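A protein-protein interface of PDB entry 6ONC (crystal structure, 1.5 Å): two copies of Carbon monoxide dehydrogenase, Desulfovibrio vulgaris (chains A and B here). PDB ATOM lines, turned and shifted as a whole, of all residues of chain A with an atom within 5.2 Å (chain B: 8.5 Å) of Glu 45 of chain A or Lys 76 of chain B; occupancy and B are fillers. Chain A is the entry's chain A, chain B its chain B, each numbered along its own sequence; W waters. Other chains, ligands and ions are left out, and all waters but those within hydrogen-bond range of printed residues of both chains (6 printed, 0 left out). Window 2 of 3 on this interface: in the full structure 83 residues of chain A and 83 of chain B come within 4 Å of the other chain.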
ATOM      1  N   ASP A  41       6.786  25.931  15.372  1.00  0.00           N
ATOM      2  CA  ASP A  41       6.534  26.397  14.012  1.00  0.00           C
ATOM      3  C   ASP A  41       5.138  26.002  13.549  1.00  0.00           C
ATOM      4  O   ASP A  41       4.448  26.790  12.887  1.00  0.00           O
ATOM      5  CB  ASP A  41       7.578  25.824  13.057  1.00  0.00           C
ATOM      6  CG  ASP A  41       8.986  26.214  13.441  1.00  0.00           C
ATOM      7  OD1 ASP A  41       9.214  27.418  13.666  1.00  0.00           O
ATOM      8  OD2 ASP A  41       9.849  25.316  13.534  1.00  0.00           O
ATOM      9  N   ARG A  42       4.715  24.782  13.878  1.00  0.00           N
ATOM     10  CA  ARG A  42       3.385  24.341  13.484  1.00  0.00           C
ATOM     11  C   ARG A  42       2.303  25.050  14.288  1.00  0.00           C
ATOM     12  O   ARG A  42       1.230  25.328  13.752  1.00  0.00           O
ATOM     13  CB  ARG A  42       3.271  22.819  13.598  1.00  0.00           C
ATOM     14  CG  ARG A  42       4.251  22.054  12.676  1.00  0.00           C
ATOM     15  CD  ARG A  42       4.003  20.546  12.731  1.00  0.00           C
ATOM     16  NE  ARG A  42       4.153  20.016  14.083  1.00  0.00           N
ATOM     17  CZ  ARG A  42       5.299  19.587  14.613  1.00  0.00           C
ATOM     18  NH1 ARG A  42       6.429  19.605  13.905  1.00  0.00           N
ATOM     19  NH2 ARG A  42       5.318  19.130  15.853  1.00  0.00           N
ATOM     20  N   ALA A  43       2.569  25.372  15.559  1.00  0.00           N
ATOM     21  CA  ALA A  43       1.614  26.172  16.321  1.00  0.00           C
ATOM     22  C   ALA A  43       1.404  27.544  15.680  1.00  0.00           C
ATOM     23  O   ALA A  43       0.275  28.051  15.637  1.00  0.00           O
ATOM     24  CB  ALA A  43       2.072  26.315  17.777  1.00  0.00           C
ATOM     25  N   ALA A  44       2.486  28.169  15.189  1.00  0.00           N
ATOM     26  CA  ALA A  44       2.342  29.453  14.504  1.00  0.00           C
ATOM     27  C   ALA A  44       1.520  29.315  13.226  1.00  0.00           C
ATOM     28  O   ALA A  44       0.723  30.204  12.899  1.00  0.00           O
ATOM     29  CB  ALA A  44       3.714  30.066  14.208  1.00  0.00           C
ATOM     30  N   GLU A  45       1.697  28.213  12.489  1.00  0.00           N
ATOM     31  CA  GLU A  45       0.893  27.989  11.285  1.00  0.00           C
ATOM     32  C   GLU A  45      -0.585  27.839  11.615  1.00  0.00           C
ATOM     33  O   GLU A  45      -1.445  28.177  10.788  1.00  0.00           O
ATOM     34  CB  GLU A  45       1.365  26.739  10.545  1.00  0.00           C
ATOM     35  CG  GLU A  45       2.742  26.857   9.922  1.00  0.00           C
ATOM     36  CD  GLU A  45       3.127  25.614   9.143  1.00  0.00           C
ATOM     37  OE1 GLU A  45       2.273  24.715   9.005  1.00  0.00           O
ATOM     38  OE2 GLU A  45       4.288  25.529   8.682  1.00  0.00           O
ATOM     39  N   GLN A  46      -0.902  27.310  12.792  1.00  0.00           N
ATOM     40  CA  GLN A  46      -2.281  27.049  13.184  1.00  0.00           C
ATOM     41  C   GLN A  46      -2.899  28.201  13.963  1.00  0.00           C
ATOM     42  O   GLN A  46      -4.008  28.057  14.497  1.00  0.00           O
ATOM     43  CB  GLN A  46      -2.367  25.747  13.985  1.00  0.00           C
ATOM     44  CG  GLN A  46      -2.015  24.497  13.191  1.00  0.00           C
ATOM     45  CD  GLN A  46      -3.059  24.149  12.126  1.00  0.00           C
ATOM     46  OE1 GLN A  46      -4.207  24.584  12.190  1.00  0.00           O
ATOM     47  NE2 GLN A  46      -2.650  23.364  11.140  1.00  0.00           N
ATOM     48  N   THR A  47      -2.208  29.338  14.041  1.00  0.00           N
ATOM     49  CA  THR A  47      -2.728  30.556  14.636  1.00  0.00           C
ATOM     50  C   THR A  47      -2.906  31.583  13.533  1.00  0.00           C
ATOM     51  O   THR A  47      -1.967  31.813  12.759  1.00  0.00           O
ATOM     52  CB  THR A  47      -1.724  31.079  15.669  1.00  0.00           C
ATOM     53  OG1 THR A  47      -1.463  30.048  16.629  1.00  0.00           O
ATOM     54  CG2 THR A  47      -2.283  32.299  16.385  1.00  0.00           C
ATOM     55  N   PRO B  66      -7.094  24.092  18.468  1.00  0.00           N
ATOM     56  CA  PRO B  66      -7.567  23.228  17.376  1.00  0.00           C
ATOM     57  C   PRO B  66      -6.818  23.434  16.065  1.00  0.00           C
ATOM     58  O   PRO B  66      -6.254  24.511  15.836  1.00  0.00           O
ATOM     59  CB  PRO B  66      -9.036  23.637  17.224  1.00  0.00           C
ATOM     60  CG  PRO B  66      -9.057  25.061  17.634  1.00  0.00           C
ATOM     61  CD  PRO B  66      -8.073  25.146  18.793  1.00  0.00           C
ATOM     62  N   CYS B  67      -6.811  22.412  15.216  1.00  0.00           N
ATOM     63  CA  CYS B  67      -6.003  22.413  14.007  1.00  0.00           C
ATOM     64  C   CYS B  67      -6.885  22.196  12.792  1.00  0.00           C
ATOM     65  O   CYS B  67      -7.887  21.479  12.854  1.00  0.00           O
ATOM     66  CB  CYS B  67      -4.957  21.292  14.038  1.00  0.00           C
ATOM     67  SG  CYS B  67      -3.796  21.433  15.409  1.00  0.00           S
ATOM     68  N   ARG B  68      -6.487  22.804  11.676  1.00  0.00           N
ATOM     69  CA  ARG B  68      -7.096  22.540  10.383  1.00  0.00           C
ATOM     70  C   ARG B  68      -6.002  22.156   9.401  1.00  0.00           C
ATOM     71  O   ARG B  68      -4.902  22.718   9.445  1.00  0.00           O
ATOM     72  CB  ARG B  68      -7.813  23.781   9.857  1.00  0.00           C
ATOM     73  CG  ARG B  68      -9.183  24.029  10.477  1.00  0.00           C
ATOM     74  CD  ARG B  68      -9.630  25.454  10.229  1.00  0.00           C
ATOM     75  NE  ARG B  68      -8.751  26.385  10.932  1.00  0.00           N
ATOM     76  CZ  ARG B  68      -8.453  27.604  10.500  1.00  0.00           C
ATOM     77  NH1 ARG B  68      -8.963  28.047   9.361  1.00  0.00           N
ATOM     78  NH2 ARG B  68      -7.639  28.377  11.209  1.00  0.00           N
ATOM     79  N   ILE B  69      -6.306  21.212   8.512  1.00  0.00           N
ATOM     80  CA  ILE B  69      -5.344  20.696   7.536  1.00  0.00           C
ATOM     81  C   ILE B  69      -5.750  21.188   6.156  1.00  0.00           C
ATOM     82  O   ILE B  69      -6.869  20.925   5.694  1.00  0.00           O
ATOM     83  CB  ILE B  69      -5.268  19.161   7.553  1.00  0.00           C
ATOM     84  CG1 ILE B  69      -4.870  18.660   8.934  1.00  0.00           C
ATOM     85  CG2 ILE B  69      -4.273  18.666   6.513  1.00  0.00           C
ATOM     86  CD1 ILE B  69      -3.534  19.188   9.426  1.00  0.00           C
ATOM     87  N   ALA B  70      -4.842  21.895   5.495  1.00  0.00           N
ATOM     88  CA  ALA B  70      -5.050  22.349   4.129  1.00  0.00           C
ATOM     89  C   ALA B  70      -4.122  21.598   3.182  1.00  0.00           C
ATOM     90  O   ALA B  70      -3.188  20.904   3.597  1.00  0.00           O
ATOM     91  CB  ALA B  70      -4.808  23.858   4.019  1.00  0.00           C
ATOM     92  N   ASN B  71      -4.394  21.748   1.889  1.00  0.00           N
ATOM     93  CA  ASN B  71      -3.581  21.156   0.826  1.00  0.00           C
ATOM     94  C   ASN B  71      -3.024  22.303  -0.011  1.00  0.00           C
ATOM     95  O   ASN B  71      -3.567  22.643  -1.065  1.00  0.00           O
ATOM     96  CB  ASN B  71      -4.414  20.173  -0.021  1.00  0.00           C
ATOM     97  N   ARG B  72      -1.937  22.900   0.469  1.00  0.00           N
ATOM     98  CA  ARG B  72      -1.323  24.061  -0.161  1.00  0.00           C
ATOM     99  C   ARG B  72       0.027  23.688  -0.754  1.00  0.00           C
ATOM    100  O   ARG B  72       0.767  22.878  -0.183  1.00  0.00           O
ATOM    101  CB  ARG B  72      -1.123  25.181   0.857  1.00  0.00           C
ATOM    102  CG  ARG B  72      -2.416  25.726   1.421  1.00  0.00           C
ATOM    103  CD  ARG B  72      -2.152  26.542   2.667  1.00  0.00           C
ATOM    104  NE  ARG B  72      -1.222  27.630   2.399  1.00  0.00           N
ATOM    105  CZ  ARG B  72      -1.578  28.792   1.860  1.00  0.00           C
ATOM    106  NH1 ARG B  72      -2.847  29.012   1.534  1.00  0.00           N
ATOM    107  NH2 ARG B  72      -0.667  29.734   1.647  1.00  0.00           N
ATOM    108  N   LYS B  73       0.347  24.301  -1.897  1.00  0.00           N
ATOM    109  CA  LYS B  73       1.624  24.036  -2.550  1.00  0.00           C
ATOM    110  C   LYS B  73       2.801  24.468  -1.683  1.00  0.00           C
ATOM    111  O   LYS B  73       3.876  23.853  -1.744  1.00  0.00           O
ATOM    112  CB  LYS B  73       1.669  24.738  -3.912  1.00  0.00           C
ATOM    113  N   ASP B  74       2.622  25.511  -0.868  1.00  0.00           N
ATOM    114  CA  ASP B  74       3.704  25.962  -0.002  1.00  0.00           C
ATOM    115  C   ASP B  74       3.899  25.082   1.223  1.00  0.00           C
ATOM    116  O   ASP B  74       4.857  25.299   1.971  1.00  0.00           O
ATOM    117  CB  ASP B  74       3.533  27.435   0.405  1.00  0.00           C
ATOM    118  CG  ASP B  74       2.301  27.681   1.267  1.00  0.00           C
ATOM    119  OD1 ASP B  74       1.587  26.718   1.611  1.00  0.00           O
ATOM    120  OD2 ASP B  74       2.047  28.859   1.601  1.00  0.00           O
ATOM    121  N   GLY B  75       3.018  24.106   1.451  1.00  0.00           N
ATOM    122  CA  GLY B  75       3.189  23.186   2.555  1.00  0.00           C
ATOM    123  C   GLY B  75       2.737  23.691   3.911  1.00  0.00           C
ATOM    124  O   GLY B  75       2.895  22.967   4.903  1.00  0.00           O
ATOM    125  N   LYS B  76       2.191  24.900   3.996  1.00  0.00           N
ATOM    126  CA  LYS B  76       1.709  25.408   5.274  1.00  0.00           C
ATOM    127  C   LYS B  76       0.411  24.711   5.669  1.00  0.00           C
ATOM    128  O   LYS B  76      -0.416  24.361   4.819  1.00  0.00           O
ATOM    129  CB  LYS B  76       1.478  26.916   5.194  1.00  0.00           C
ATOM    130  N   MET B  77       0.241  24.513   6.981  1.00  0.00           N
ATOM    131  CA  MET B  77      -0.952  23.870   7.543  1.00  0.00           C
ATOM    132  C   MET B  77      -1.170  22.465   6.985  1.00  0.00           C
ATOM    133  O   MET B  77      -2.301  21.983   6.900  1.00  0.00           O
ATOM    134  CB  MET B  77      -2.207  24.735   7.400  1.00  0.00           C
ATOM    135  CG  MET B  77      -2.137  26.027   8.204  1.00  0.00           C
ATOM    136  SD  MET B  77      -3.564  27.097   7.978  1.00  0.00           S
ATOM    137  CE  MET B  77      -4.802  26.251   8.971  1.00  0.00           C
ATOM    138  N   ARG B  78      -0.088  21.808   6.580  1.00  0.00           N
ATOM    139  CA  ARG B  78      -0.164  20.417   6.167  1.00  0.00           C
ATOM    140  C   ARG B  78      -0.301  19.490   7.365  1.00  0.00           C
ATOM    141  O   ARG B  78      -0.842  18.383   7.234  1.00  0.00           O
ATOM    142  CB  ARG B  78       1.088  20.058   5.352  1.00  0.00           C
ATOM    143  CG  ARG B  78       1.095  18.651   4.779  1.00  0.00           C
ATOM    144  CD  ARG B  78       2.330  18.397   3.926  1.00  0.00           C
ATOM    145  NE  ARG B  78       3.559  18.418   4.716  1.00  0.00           N
ATOM    146  CZ  ARG B  78       4.081  17.356   5.324  1.00  0.00           C
ATOM    147  NH1 ARG B  78       5.201  17.481   6.029  1.00  0.00           N
ATOM    148  NH2 ARG B  78       3.480  16.176   5.240  1.00  0.00           N
ATOM    149  N   LEU B  79       0.175  19.917   8.534  1.00  0.00           N
ATOM    150  CA  LEU B  79       0.191  19.074   9.718  1.00  0.00           C
ATOM    151  C   LEU B  79      -0.414  19.819  10.902  1.00  0.00           C
ATOM    152  O   LEU B  79      -0.362  21.052  10.986  1.00  0.00           O
ATOM    153  CB  LEU B  79       1.628  18.682  10.107  1.00  0.00           C
ATOM    154  CG  LEU B  79       2.440  18.024   8.990  1.00  0.00           C
ATOM    155  CD1 LEU B  79       3.880  17.837   9.435  1.00  0.00           C
ATOM    156  CD2 LEU B  79       1.820  16.702   8.556  1.00  0.00           C
ATOM    157  N   GLY B  80      -0.977  19.050  11.827  1.00  0.00           N
ATOM    158  CA  GLY B  80      -1.413  19.608  13.083  1.00  0.00           C
ATOM    159  C   GLY B  80      -0.221  20.008  13.935  1.00  0.00           C
ATOM    160  O   GLY B  80       0.941  19.736  13.616  1.00  0.00           O
ATOM    161  N   VAL B  81      -0.512  20.678  15.050  1.00  0.00           N
ATOM    162  CA  VAL B  81       0.581  21.149  15.902  1.00  0.00           C
ATOM    163  C   VAL B  81       1.438  19.980  16.370  1.00  0.00           C
ATOM    164  O   VAL B  81       2.671  20.080  16.421  1.00  0.00           O
ATOM    165  CB  VAL B  81       0.048  22.005  17.063  1.00  0.00           C
ATOM    166  CG1 VAL B  81       1.203  22.419  17.997  1.00  0.00           C
ATOM    167  CG2 VAL B  81      -0.665  23.241  16.522  1.00  0.00           C
HETATM  168  O   HOH W   1      -0.750  29.472   8.368  1.00  0.00           O
HETATM  169  O   HOH W   2      -4.151  29.460  10.831  1.00  0.00           O
HETATM  170  O   HOH W   3       2.441  22.120   8.416  1.00  0.00           O
HETATM  171  O   HOH W   4       0.569  23.531  10.613  1.00  0.00           O
HETATM  172  O   HOH W   5      -5.803  26.671  12.959  1.00  0.00           O
HETATM  173  O   HOH W   6      -4.612  26.380  16.783  1.00  0.00           O
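The side-chain amide nitrogen (NE2) of Gln 46 of chain A sits at hydrogen-bond distance from the backbone carbonyl oxygen (O) of Leu 79 of chain B, 3.3 Å away. N of Met 77 of chain B sits at hydrogen-bond distance from OE1 of Glu 45 of chain A, 2.9 Å away. O of Val 81 of chain B sits at hydrogen-bond distance from NE of Arg 42 of chain A, 2.8 Å away. The side-chain amide nitrogen of Gln 46 of chain A lies within hydrogen-bond range of the backbone carbonyl oxygen of Arg 68 of chain B (2.9 Å). NE of Arg 42 of chain A sits at hydrogen-bond distance from O of Gly 80 of chain B, 3.3 Å away.
N of Val 81 of chain B lies close to SG of Cys 67 of chain B (3.4 Å). N of Ala 70 of chain B sits at hydrogen-bond distance from O of Met 77 of chain B, 2.9 Å away. OG1 of Thr 47 of chain A sits at hydrogen-bond distance from O of Ala 43 of chain A (2.8 Å). OD1 of Asp 74 of chain B is in hydrogen-bond range of N of Lys 76 of chain B (3.1 Å).
Ala 43 of chain A touches Val 81 of chain B (CA to CG2, 3.7 Å). Glu 45 of chain A touches Lys 76 of chain B. Gln 46 of chain A touches Cys 67 of chain B. Gln 46 of chain A touches Met 77 of chain B (OE1 to CE, 3.7 Å). Gln 46 of chain A touches Val 81 of chain B.
No residue of chain B comes within 4 Å of Ala 44 of chain A. Of the printed residues of chain B, Gln 46 of chain A touches Cys 67, Arg 68, Met 77, Leu 79 and Val 81. Printed residues of chain A within 4 Å of Cys 67 of chain B: Gln 46 (3.4 Å). Asn 71 of chain B touches none of the printed residues of chain A. Printed residues of chain A within 4 Å of Lys 76 of chain B: Glu 45 (3.8 Å). Of the printed residues of chain A, Met 77 of chain B touches Glu 45 and Gln 46. Printed residues of chain A within 4 Å of Leu 79 of chain B: Gln 46. The nearest printed residue of chain B that does not touch Gln 46 of chain A is Pro 66 of chain B (4.2 Å).
Printed residues of chain B that touch a printed residue of chain A: Cys 67, Arg 68, Lys 76, Met 77, Leu 79, Gly 80 and Val 81. Hydrophobic or aromatic side chains of chain B that line the printed part of chain A: Met 77 and Val 81. Printed residues of chain A that touch a printed residue of chain B: Arg 42, Ala 43, Glu 45 and Gln 46. Hydrophobic or aromatic side chains of chain A within 4 Å of the printed part of chain B: Ala 43. Among the printed residues, 10 pairs touch across the chains. Among the printed residues, no Asp or Glu carboxylate lies within 4 Å of a Lys or Arg side-chain nitrogen of the other chain.
No position is printed for both chains. Of the 10 pairs that touch across the chains among the printed residues, none has its exchanged pair printed and touching as well.
Water W4 lies within hydrogen-bond range of OE1 of Glu 45 of chain A (2.6 Å), O of Leu 79 of chain B (2.7 Å) and NE2 of Gln 46 of chain A (3.3 Å). Water W6 lies within hydrogen-bond range of the backbone carbonyl oxygen of Pro 66 of chain B and the backbone carbonyl oxygen of Gln 46 of chain A. Water W3 lies within hydrogen-bond range of the side-chain carboxylate of Glu 45 of chain A (2.7 Å), the backbone NH of Arg 78 of chain B (3.1 Å) and the backbone NH of Leu 79 of chain B (3.2 Å). Water W5 bridges the side-chain amide oxygen of Gln 46 of chain A (2.7 Å) and the guanidinium group of Arg 68 of chain B (3.1 Å). Water W1 lies within hydrogen-bond range of O of Glu 45 of chain A (2.8 Å) and SD of Met 77 of chain B (3.7 Å). Water W2 lies within hydrogen-bond range of O of Glu 45 of chain A and SD of Met 77 of chain B.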
